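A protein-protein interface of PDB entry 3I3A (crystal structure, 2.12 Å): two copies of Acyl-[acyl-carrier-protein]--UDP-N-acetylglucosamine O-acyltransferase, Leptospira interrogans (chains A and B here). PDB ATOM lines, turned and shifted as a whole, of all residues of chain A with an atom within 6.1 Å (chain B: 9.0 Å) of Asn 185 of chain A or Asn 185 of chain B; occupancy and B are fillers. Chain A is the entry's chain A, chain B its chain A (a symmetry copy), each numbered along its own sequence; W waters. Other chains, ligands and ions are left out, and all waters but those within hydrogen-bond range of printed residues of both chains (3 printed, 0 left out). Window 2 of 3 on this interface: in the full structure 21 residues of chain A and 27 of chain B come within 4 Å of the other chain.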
ATOM      1  N   GLY A 168      23.284  31.415 -21.526  1.00  0.00           N
ATOM      2  CA  GLY A 168      22.110  30.549 -21.519  1.00  0.00           C
ATOM      3  C   GLY A 168      22.472  29.082 -21.341  1.00  0.00           C
ATOM      4  O   GLY A 168      23.389  28.587 -21.988  1.00  0.00           O
ATOM      5  N   LEU A 169      21.764  28.398 -20.439  1.00  0.00           N
ATOM      6  CA  LEU A 169      21.888  26.937 -20.286  1.00  0.00           C
ATOM      7  C   LEU A 169      23.250  26.435 -19.782  1.00  0.00           C
ATOM      8  O   LEU A 169      23.554  25.244 -19.880  1.00  0.00           O
ATOM      9  CB  LEU A 169      21.489  26.206 -21.591  1.00  0.00           C
ATOM     10  CG  LEU A 169      19.979  26.042 -21.827  1.00  0.00           C
ATOM     11  CD1 LEU A 169      19.654  25.839 -23.281  1.00  0.00           C
ATOM     12  CD2 LEU A 169      19.409  24.877 -21.028  1.00  0.00           C
ATOM     13  N   ALA A 170      24.065  27.323 -19.231  1.00  0.00           N
ATOM     14  CA  ALA A 170      25.363  26.900 -18.704  1.00  0.00           C
ATOM     15  C   ALA A 170      25.167  26.093 -17.421  1.00  0.00           C
ATOM     16  O   ALA A 170      24.294  26.401 -16.589  1.00  0.00           O
ATOM     17  CB  ALA A 170      26.284  28.111 -18.452  1.00  0.00           C
ATOM     18  N   LYS A 171      25.975  25.049 -17.275  1.00  0.00           N
ATOM     19  CA  LYS A 171      25.959  24.251 -16.069  1.00  0.00           C
ATOM     20  C   LYS A 171      27.163  24.665 -15.240  1.00  0.00           C
ATOM     21  O   LYS A 171      28.299  24.326 -15.563  1.00  0.00           O
ATOM     22  CB  LYS A 171      25.991  22.738 -16.401  1.00  0.00           C
ATOM     23  CG  LYS A 171      25.952  21.815 -15.167  1.00  0.00           C
ATOM     24  CD  LYS A 171      26.703  20.489 -15.447  1.00  0.00           C
ATOM     25  CE  LYS A 171      26.656  19.542 -14.242  1.00  0.00           C
ATOM     26  NZ  LYS A 171      27.615  18.403 -14.379  1.00  0.00           N
ATOM     27  N   ASP A 183      30.409  29.795 -20.008  1.00  0.00           N
ATOM     28  CA  ASP A 183      29.477  29.177 -20.952  1.00  0.00           C
ATOM     29  C   ASP A 183      29.694  27.672 -21.129  1.00  0.00           C
ATOM     30  O   ASP A 183      30.837  27.179 -21.130  1.00  0.00           O
ATOM     31  CB  ASP A 183      29.568  29.885 -22.317  1.00  0.00           C
ATOM     32  CG  ASP A 183      28.669  29.259 -23.364  1.00  0.00           C
ATOM     33  OD1 ASP A 183      27.430  29.240 -23.190  1.00  0.00           O
ATOM     34  OD2 ASP A 183      29.201  28.789 -24.380  1.00  0.00           O
ATOM     35  N   GLY A 184      28.581  26.957 -21.290  1.00  0.00           N
ATOM     36  CA  GLY A 184      28.605  25.572 -21.765  1.00  0.00           C
ATOM     37  C   GLY A 184      28.187  24.517 -20.756  1.00  0.00           C
ATOM     38  O   GLY A 184      27.838  24.818 -19.603  1.00  0.00           O
ATOM     39  N   ASN A 185      28.221  23.273 -21.215  1.00  0.00           N
ATOM     40  CA  ASN A 185      28.087  22.090 -20.364  1.00  0.00           C
ATOM     41  C   ASN A 185      28.995  20.995 -20.937  1.00  0.00           C
ATOM     42  O   ASN A 185      28.632  20.362 -21.929  1.00  0.00           O
ATOM     43  CB  ASN A 185      26.623  21.624 -20.305  1.00  0.00           C
ATOM     44  CG  ASN A 185      26.438  20.308 -19.529  1.00  0.00           C
ATOM     45  OD1 ASN A 185      27.373  19.783 -18.921  1.00  0.00           O
ATOM     46  ND2 ASN A 185      25.219  19.773 -19.561  1.00  0.00           N
ATOM     47  N   PRO A 186      30.187  20.776 -20.330  1.00  0.00           N
ATOM     48  CA  PRO A 186      30.691  21.476 -19.148  1.00  0.00           C
ATOM     49  C   PRO A 186      31.031  22.932 -19.444  1.00  0.00           C
ATOM     50  O   PRO A 186      31.491  23.261 -20.547  1.00  0.00           O
ATOM     51  CB  PRO A 186      31.961  20.698 -18.777  1.00  0.00           C
ATOM     52  CG  PRO A 186      32.392  20.025 -20.021  1.00  0.00           C
ATOM     53  CD  PRO A 186      31.153  19.781 -20.844  1.00  0.00           C
ATOM     54  N   SER A 187      30.784  23.790 -18.459  1.00  0.00           N
ATOM     55  CA  SER A 187      31.040  25.216 -18.603  1.00  0.00           C
ATOM     56  C   SER A 187      32.530  25.529 -18.468  1.00  0.00           C
ATOM     57  O   SER A 187      33.280  24.806 -17.791  1.00  0.00           O
ATOM     58  CB  SER A 187      30.239  26.012 -17.579  1.00  0.00           C
ATOM     59  OG  SER A 187      30.668  25.684 -16.274  1.00  0.00           O
ATOM     60  N   LEU B 151      12.933  22.481 -22.368  1.00  0.00           N
ATOM     61  CA  LEU B 151      14.073  23.200 -21.778  1.00  0.00           C
ATOM     62  C   LEU B 151      15.079  23.742 -22.807  1.00  0.00           C
ATOM     63  O   LEU B 151      16.280  23.792 -22.567  1.00  0.00           O
ATOM     64  CB  LEU B 151      14.756  22.363 -20.679  1.00  0.00           C
ATOM     65  CG  LEU B 151      13.893  21.875 -19.502  1.00  0.00           C
ATOM     66  CD1 LEU B 151      14.718  21.094 -18.488  1.00  0.00           C
ATOM     67  CD2 LEU B 151      13.181  23.026 -18.814  1.00  0.00           C
ATOM     68  N   ALA B 153      16.420  27.035 -24.851  1.00  0.00           N
ATOM     69  CA  ALA B 153      16.474  28.481 -24.824  1.00  0.00           C
ATOM     70  C   ALA B 153      16.828  29.014 -26.226  1.00  0.00           C
ATOM     71  O   ALA B 153      17.835  28.615 -26.817  1.00  0.00           O
ATOM     72  CB  ALA B 153      17.485  28.945 -23.800  1.00  0.00           C
ATOM     73  N   ALA B 167      15.917  20.118 -30.569  1.00  0.00           N
ATOM     74  CA  ALA B 167      15.996  19.033 -29.576  1.00  0.00           C
ATOM     75  C   ALA B 167      16.045  19.523 -28.139  1.00  0.00           C
ATOM     76  O   ALA B 167      16.399  20.682 -27.884  1.00  0.00           O
ATOM     77  CB  ALA B 167      17.206  18.184 -29.844  1.00  0.00           C
ATOM     78  N   GLY B 168      15.695  18.631 -27.206  1.00  0.00           N
ATOM     79  CA  GLY B 168      15.698  18.942 -25.779  1.00  0.00           C
ATOM     80  C   GLY B 168      16.972  19.646 -25.341  1.00  0.00           C
ATOM     81  O   GLY B 168      18.067  19.234 -25.711  1.00  0.00           O
ATOM     82  N   LEU B 169      16.823  20.729 -24.574  1.00  0.00           N
ATOM     83  CA  LEU B 169      17.967  21.405 -23.937  1.00  0.00           C
ATOM     84  C   LEU B 169      18.964  22.071 -24.899  1.00  0.00           C
ATOM     85  O   LEU B 169      20.080  22.418 -24.504  1.00  0.00           O
ATOM     86  CB  LEU B 169      18.705  20.453 -22.965  1.00  0.00           C
ATOM     87  CG  LEU B 169      18.054  20.279 -21.583  1.00  0.00           C
ATOM     88  CD1 LEU B 169      18.473  18.996 -20.920  1.00  0.00           C
ATOM     89  CD2 LEU B 169      18.382  21.442 -20.656  1.00  0.00           C
ATOM     90  N   ALA B 170      18.572  22.268 -26.149  1.00  0.00           N
ATOM     91  CA  ALA B 170      19.465  22.926 -27.104  1.00  0.00           C
ATOM     92  C   ALA B 170      19.581  24.413 -26.770  1.00  0.00           C
ATOM     93  O   ALA B 170      18.598  25.067 -26.374  1.00  0.00           O
ATOM     94  CB  ALA B 170      18.976  22.728 -28.553  1.00  0.00           C
ATOM     95  N   LYS B 171      20.792  24.939 -26.917  1.00  0.00           N
ATOM     96  CA  LYS B 171      21.026  26.353 -26.721  1.00  0.00           C
ATOM     97  C   LYS B 171      21.130  26.984 -28.099  1.00  0.00           C
ATOM     98  O   LYS B 171      22.129  26.819 -28.796  1.00  0.00           O
ATOM     99  CB  LYS B 171      22.307  26.596 -25.886  1.00  0.00           C
ATOM    100  CG  LYS B 171      22.614  28.081 -25.611  1.00  0.00           C
ATOM    101  CD  LYS B 171      24.141  28.312 -25.478  1.00  0.00           C
ATOM    102  CE  LYS B 171      24.472  29.778 -25.179  1.00  0.00           C
ATOM    103  NZ  LYS B 171      25.928  30.076 -25.344  1.00  0.00           N
ATOM    104  N   VAL B 172      20.085  27.695 -28.500  1.00  0.00           N
ATOM    105  CA  VAL B 172      20.021  28.261 -29.841  1.00  0.00           C
ATOM    106  C   VAL B 172      20.466  29.717 -29.806  1.00  0.00           C
ATOM    107  O   VAL B 172      19.839  30.541 -29.137  1.00  0.00           O
ATOM    108  CB  VAL B 172      18.591  28.154 -30.435  1.00  0.00           C
ATOM    109  CG1 VAL B 172      18.542  28.719 -31.858  1.00  0.00           C
ATOM    110  CG2 VAL B 172      18.110  26.706 -30.419  1.00  0.00           C
ATOM    111  N   VAL B 173      21.552  30.015 -30.523  1.00  0.00           N
ATOM    112  CA  VAL B 173      22.114  31.367 -30.593  1.00  0.00           C
ATOM    113  C   VAL B 173      22.042  31.991 -31.991  1.00  0.00           C
ATOM    114  O   VAL B 173      22.275  33.187 -32.149  1.00  0.00           O
ATOM    115  CB  VAL B 173      23.571  31.412 -30.068  1.00  0.00           C
ATOM    116  CG1 VAL B 173      23.618  31.169 -28.523  1.00  0.00           C
ATOM    117  CG2 VAL B 173      24.451  30.424 -30.795  1.00  0.00           C
ATOM    118  N   VAL B 182      18.062  20.916 -35.111  1.00  0.00           N
ATOM    119  CA  VAL B 182      19.153  21.559 -34.387  1.00  0.00           C
ATOM    120  C   VAL B 182      19.251  20.947 -32.991  1.00  0.00           C
ATOM    121  O   VAL B 182      18.226  20.678 -32.336  1.00  0.00           O
ATOM    122  CB  VAL B 182      18.963  23.106 -34.343  1.00  0.00           C
ATOM    123  CG1 VAL B 182      19.923  23.758 -33.376  1.00  0.00           C
ATOM    124  CG2 VAL B 182      19.147  23.697 -35.738  1.00  0.00           C
ATOM    125  N   ASP B 183      20.481  20.707 -32.542  1.00  0.00           N
ATOM    126  CA  ASP B 183      20.721  20.044 -31.260  1.00  0.00           C
ATOM    127  C   ASP B 183      22.053  20.430 -30.611  1.00  0.00           C
ATOM    128  O   ASP B 183      23.074  20.621 -31.297  1.00  0.00           O
ATOM    129  CB  ASP B 183      20.648  18.515 -31.438  1.00  0.00           C
ATOM    130  CG  ASP B 183      20.944  17.760 -30.158  1.00  0.00           C
ATOM    131  OD1 ASP B 183      20.207  17.916 -29.159  1.00  0.00           O
ATOM    132  OD2 ASP B 183      21.915  16.991 -30.149  1.00  0.00           O
ATOM    133  N   GLY B 184      22.025  20.529 -29.283  1.00  0.00           N
ATOM    134  CA  GLY B 184      23.247  20.593 -28.479  1.00  0.00           C
ATOM    135  C   GLY B 184      23.512  21.914 -27.778  1.00  0.00           C
ATOM    136  O   GLY B 184      22.731  22.874 -27.876  1.00  0.00           O
ATOM    137  N   ASN B 185      24.627  21.941 -27.061  1.00  0.00           N
ATOM    138  CA  ASN B 185      25.199  23.163 -26.494  1.00  0.00           C
ATOM    139  C   ASN B 185      26.727  23.039 -26.555  1.00  0.00           C
ATOM    140  O   ASN B 185      27.313  22.342 -25.725  1.00  0.00           O
ATOM    141  CB  ASN B 185      24.716  23.374 -25.049  1.00  0.00           C
ATOM    142  CG  ASN B 185      25.383  24.574 -24.357  1.00  0.00           C
ATOM    143  OD1 ASN B 185      26.126  25.342 -24.974  1.00  0.00           O
ATOM    144  ND2 ASN B 185      25.118  24.727 -23.061  1.00  0.00           N
ATOM    145  N   PRO B 186      27.380  23.695 -27.544  1.00  0.00           N
ATOM    146  CA  PRO B 186      26.762  24.546 -28.565  1.00  0.00           C
ATOM    147  C   PRO B 186      25.927  23.742 -29.553  1.00  0.00           C
ATOM    148  O   PRO B 186      26.272  22.599 -29.889  1.00  0.00           O
ATOM    149  CB  PRO B 186      27.960  25.187 -29.278  1.00  0.00           C
ATOM    150  CG  PRO B 186      29.101  24.278 -29.033  1.00  0.00           C
ATOM    151  CD  PRO B 186      28.844  23.588 -27.718  1.00  0.00           C
ATOM    152  N   SER B 187      24.826  24.343 -29.996  1.00  0.00           N
ATOM    153  CA  SER B 187      23.920  23.691 -30.930  1.00  0.00           C
ATOM    154  C   SER B 187      24.476  23.718 -32.354  1.00  0.00           C
ATOM    155  O   SER B 187      25.245  24.619 -32.727  1.00  0.00           O
ATOM    156  CB  SER B 187      22.544  24.346 -30.889  1.00  0.00           C
ATOM    157  OG  SER B 187      22.636  25.685 -31.329  1.00  0.00           O
ATOM    158  N   THR B 188      24.089  22.703 -33.120  1.00  0.00           N
ATOM    159  CA  THR B 188      24.444  22.562 -34.527  1.00  0.00           C
ATOM    160  C   THR B 188      23.233  22.051 -35.295  1.00  0.00           C
ATOM    161  O   THR B 188      22.305  21.471 -34.709  1.00  0.00           O
ATOM    162  CB  THR B 188      25.603  21.566 -34.739  1.00  0.00           C
ATOM    163  OG1 THR B 188      25.386  20.394 -33.928  1.00  0.00           O
ATOM    164  CG2 THR B 188      26.944  22.209 -34.378  1.00  0.00           C
ATOM    165  N   ARG B 259      26.659  20.516 -38.026  1.00  0.00           N
ATOM    166  CA  ARG B 259      27.425  19.480 -37.357  1.00  0.00           C
ATOM    167  C   ARG B 259      28.422  18.853 -38.332  1.00  0.00           C
ATOM    168  O   ARG B 259      28.162  18.820 -39.543  1.00  0.00           O
ATOM    169  CB  ARG B 259      26.446  18.423 -36.866  1.00  0.00           C
ATOM    170  CG  ARG B 259      26.850  17.666 -35.646  1.00  0.00           C
ATOM    171  CD  ARG B 259      25.629  17.592 -34.770  1.00  0.00           C
ATOM    172  NE  ARG B 259      25.500  16.315 -34.103  1.00  0.00           N
ATOM    173  CZ  ARG B 259      24.821  16.118 -32.978  1.00  0.00           C
ATOM    174  NH1 ARG B 259      24.776  14.900 -32.470  1.00  0.00           N
ATOM    175  NH2 ARG B 259      24.215  17.128 -32.352  1.00  0.00           N
ATOM    176  OXT ARG B 259      29.504  18.378 -37.948  1.00  0.00           O
HETATM  177  O   HOH W   1      23.728  23.180 -21.133  1.00  0.00           O
HETATM  178  O   HOH W   2      27.922  26.995 -26.020  1.00  0.00           O
HETATM  179  O   HOH W   3      29.185  23.139 -23.939  1.00  0.00           O
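Of the 9 printed residues of chain A, 5 touch a printed residue of chain B.
Of the 17 printed residues of chain B, 6 touch a printed residue of chain A.
Among the printed residues, Asp or Glu carboxylates within 4 Å of a Lys or Arg side-chain nitrogen of the other chain: Asp 183 of chain A with Lys 171 of chain B (2.8 Å).
Printed residues of chain B within 4 Å of Asp 183 of chain A: Lys 171.
Asn 185 of chain A touches one residue of chain B.
No residue of chain B comes within 4 Å of Pro 186 of chain A.
Of the printed residues of chain A, Lys 171 of chain B touches Gly 168 (3.6 Å), Leu 169 (3.7 Å) and Asp 183 (2.8 Å).
Asn 185 of chain B touches three residues of chain A.
The nearest residue of chain A that does not touch Asn 185 of chain B is Gly 168 of chain A (4.4 Å).
Water W1 lies within hydrogen-bond range of the backbone carbonyl oxygen of Leu 169 of chain A (2.4 Å) and the side-chain amide nitrogen of Asn 185 of chain B (2.8 Å).
Water W2 bridges the side-chain amide oxygen (OD1) of Asn 185 of chain B (2.7 Å) and the side-chain carboxylate (OD2) of Asp 183 of chain A (2.7 Å).
Water W3 lies within hydrogen-bond range of O of Asn 185 of chain B (2.7 Å) and N of Asn 185 of chain A (2.9 Å).
Gly 168 of chain A touches Lys 171 of chain B, but with the chains exchanged Lys 171 of chain A does not touch Gly 168 of chain B (12.7 Å).
Leu 169 of chain A touches its own counterpart, Leu 169 of chain B.
Leu 169 of chain A touches Ala 170 of chain B, but with the chains exchanged Ala 170 of chain A does not touch Leu 169 of chain B (8.2 Å).
Asp 183 of chain A touches Lys 171 of chain B, but with the chains exchanged Lys 171 of chain A does not touch Asp 183 of chain B (14.6 Å).
Positions printed for both chains: 168, 169, 170, 171, 183, 184, 185, 186 and 187.
Of the 10 pairs that touch across the chains among the printed residues, 2 have their exchanged pair printed and touching as well.
OD1 of Asp 183 of chain A lies within salt-bridge range of NZ of Lys 171 of chain B, at 2.8 Å.
Lys 171 of chain B touches Gly 168 of chain A (CE to O, 3.6 Å).
Leu 169 of chain A touches Leu 151 of chain B.
Leu 169 of chain A touches Ala 153 of chain B.
Leu 169 of chain A touches Leu 169 of chain B (CD2 to CD2, 3.6 Å).
Leu 169 of chain A touches Ala 170 of chain B.
CD1 of Leu 169 of chain A touches CA of Lys 171 of chain B (3.7 Å).
Asn 185 of chain B touches Leu 169 of chain A (ND2 to O, 3.6 Å).
CA of Gly 184 of chain A touches ND2 of Asn 185 of chain B, at 3.8 Å.
N of Asn 185 of chain A touches ND2 of Asn 185 of chain B, at 3.9 Å.
N of Lys 171 of chain B is in hydrogen-bond range of O of Gly 184 of chain B (3.0 Å).
The backbone carbonyl oxygen (O) of Ala 153 of chain B is in hydrogen-bond range of the backbone NH (N) of Val 172 of chain B.
The backbone NH (N) of Lys 171 of chain A is in hydrogen-bond range of the backbone carbonyl oxygen (O) of Gly 184 of chain A, 3.0 Å away.
The backbone carbonyl oxygen of Ala 170 of chain B sits at hydrogen-bond distance from the backbone NH of Ala 153 of chain B, 3.3 Å away.
OG of Ser 187 of chain B lies within hydrogen-bond range of O of Lys 171 of chain B, 2.8 Å away.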
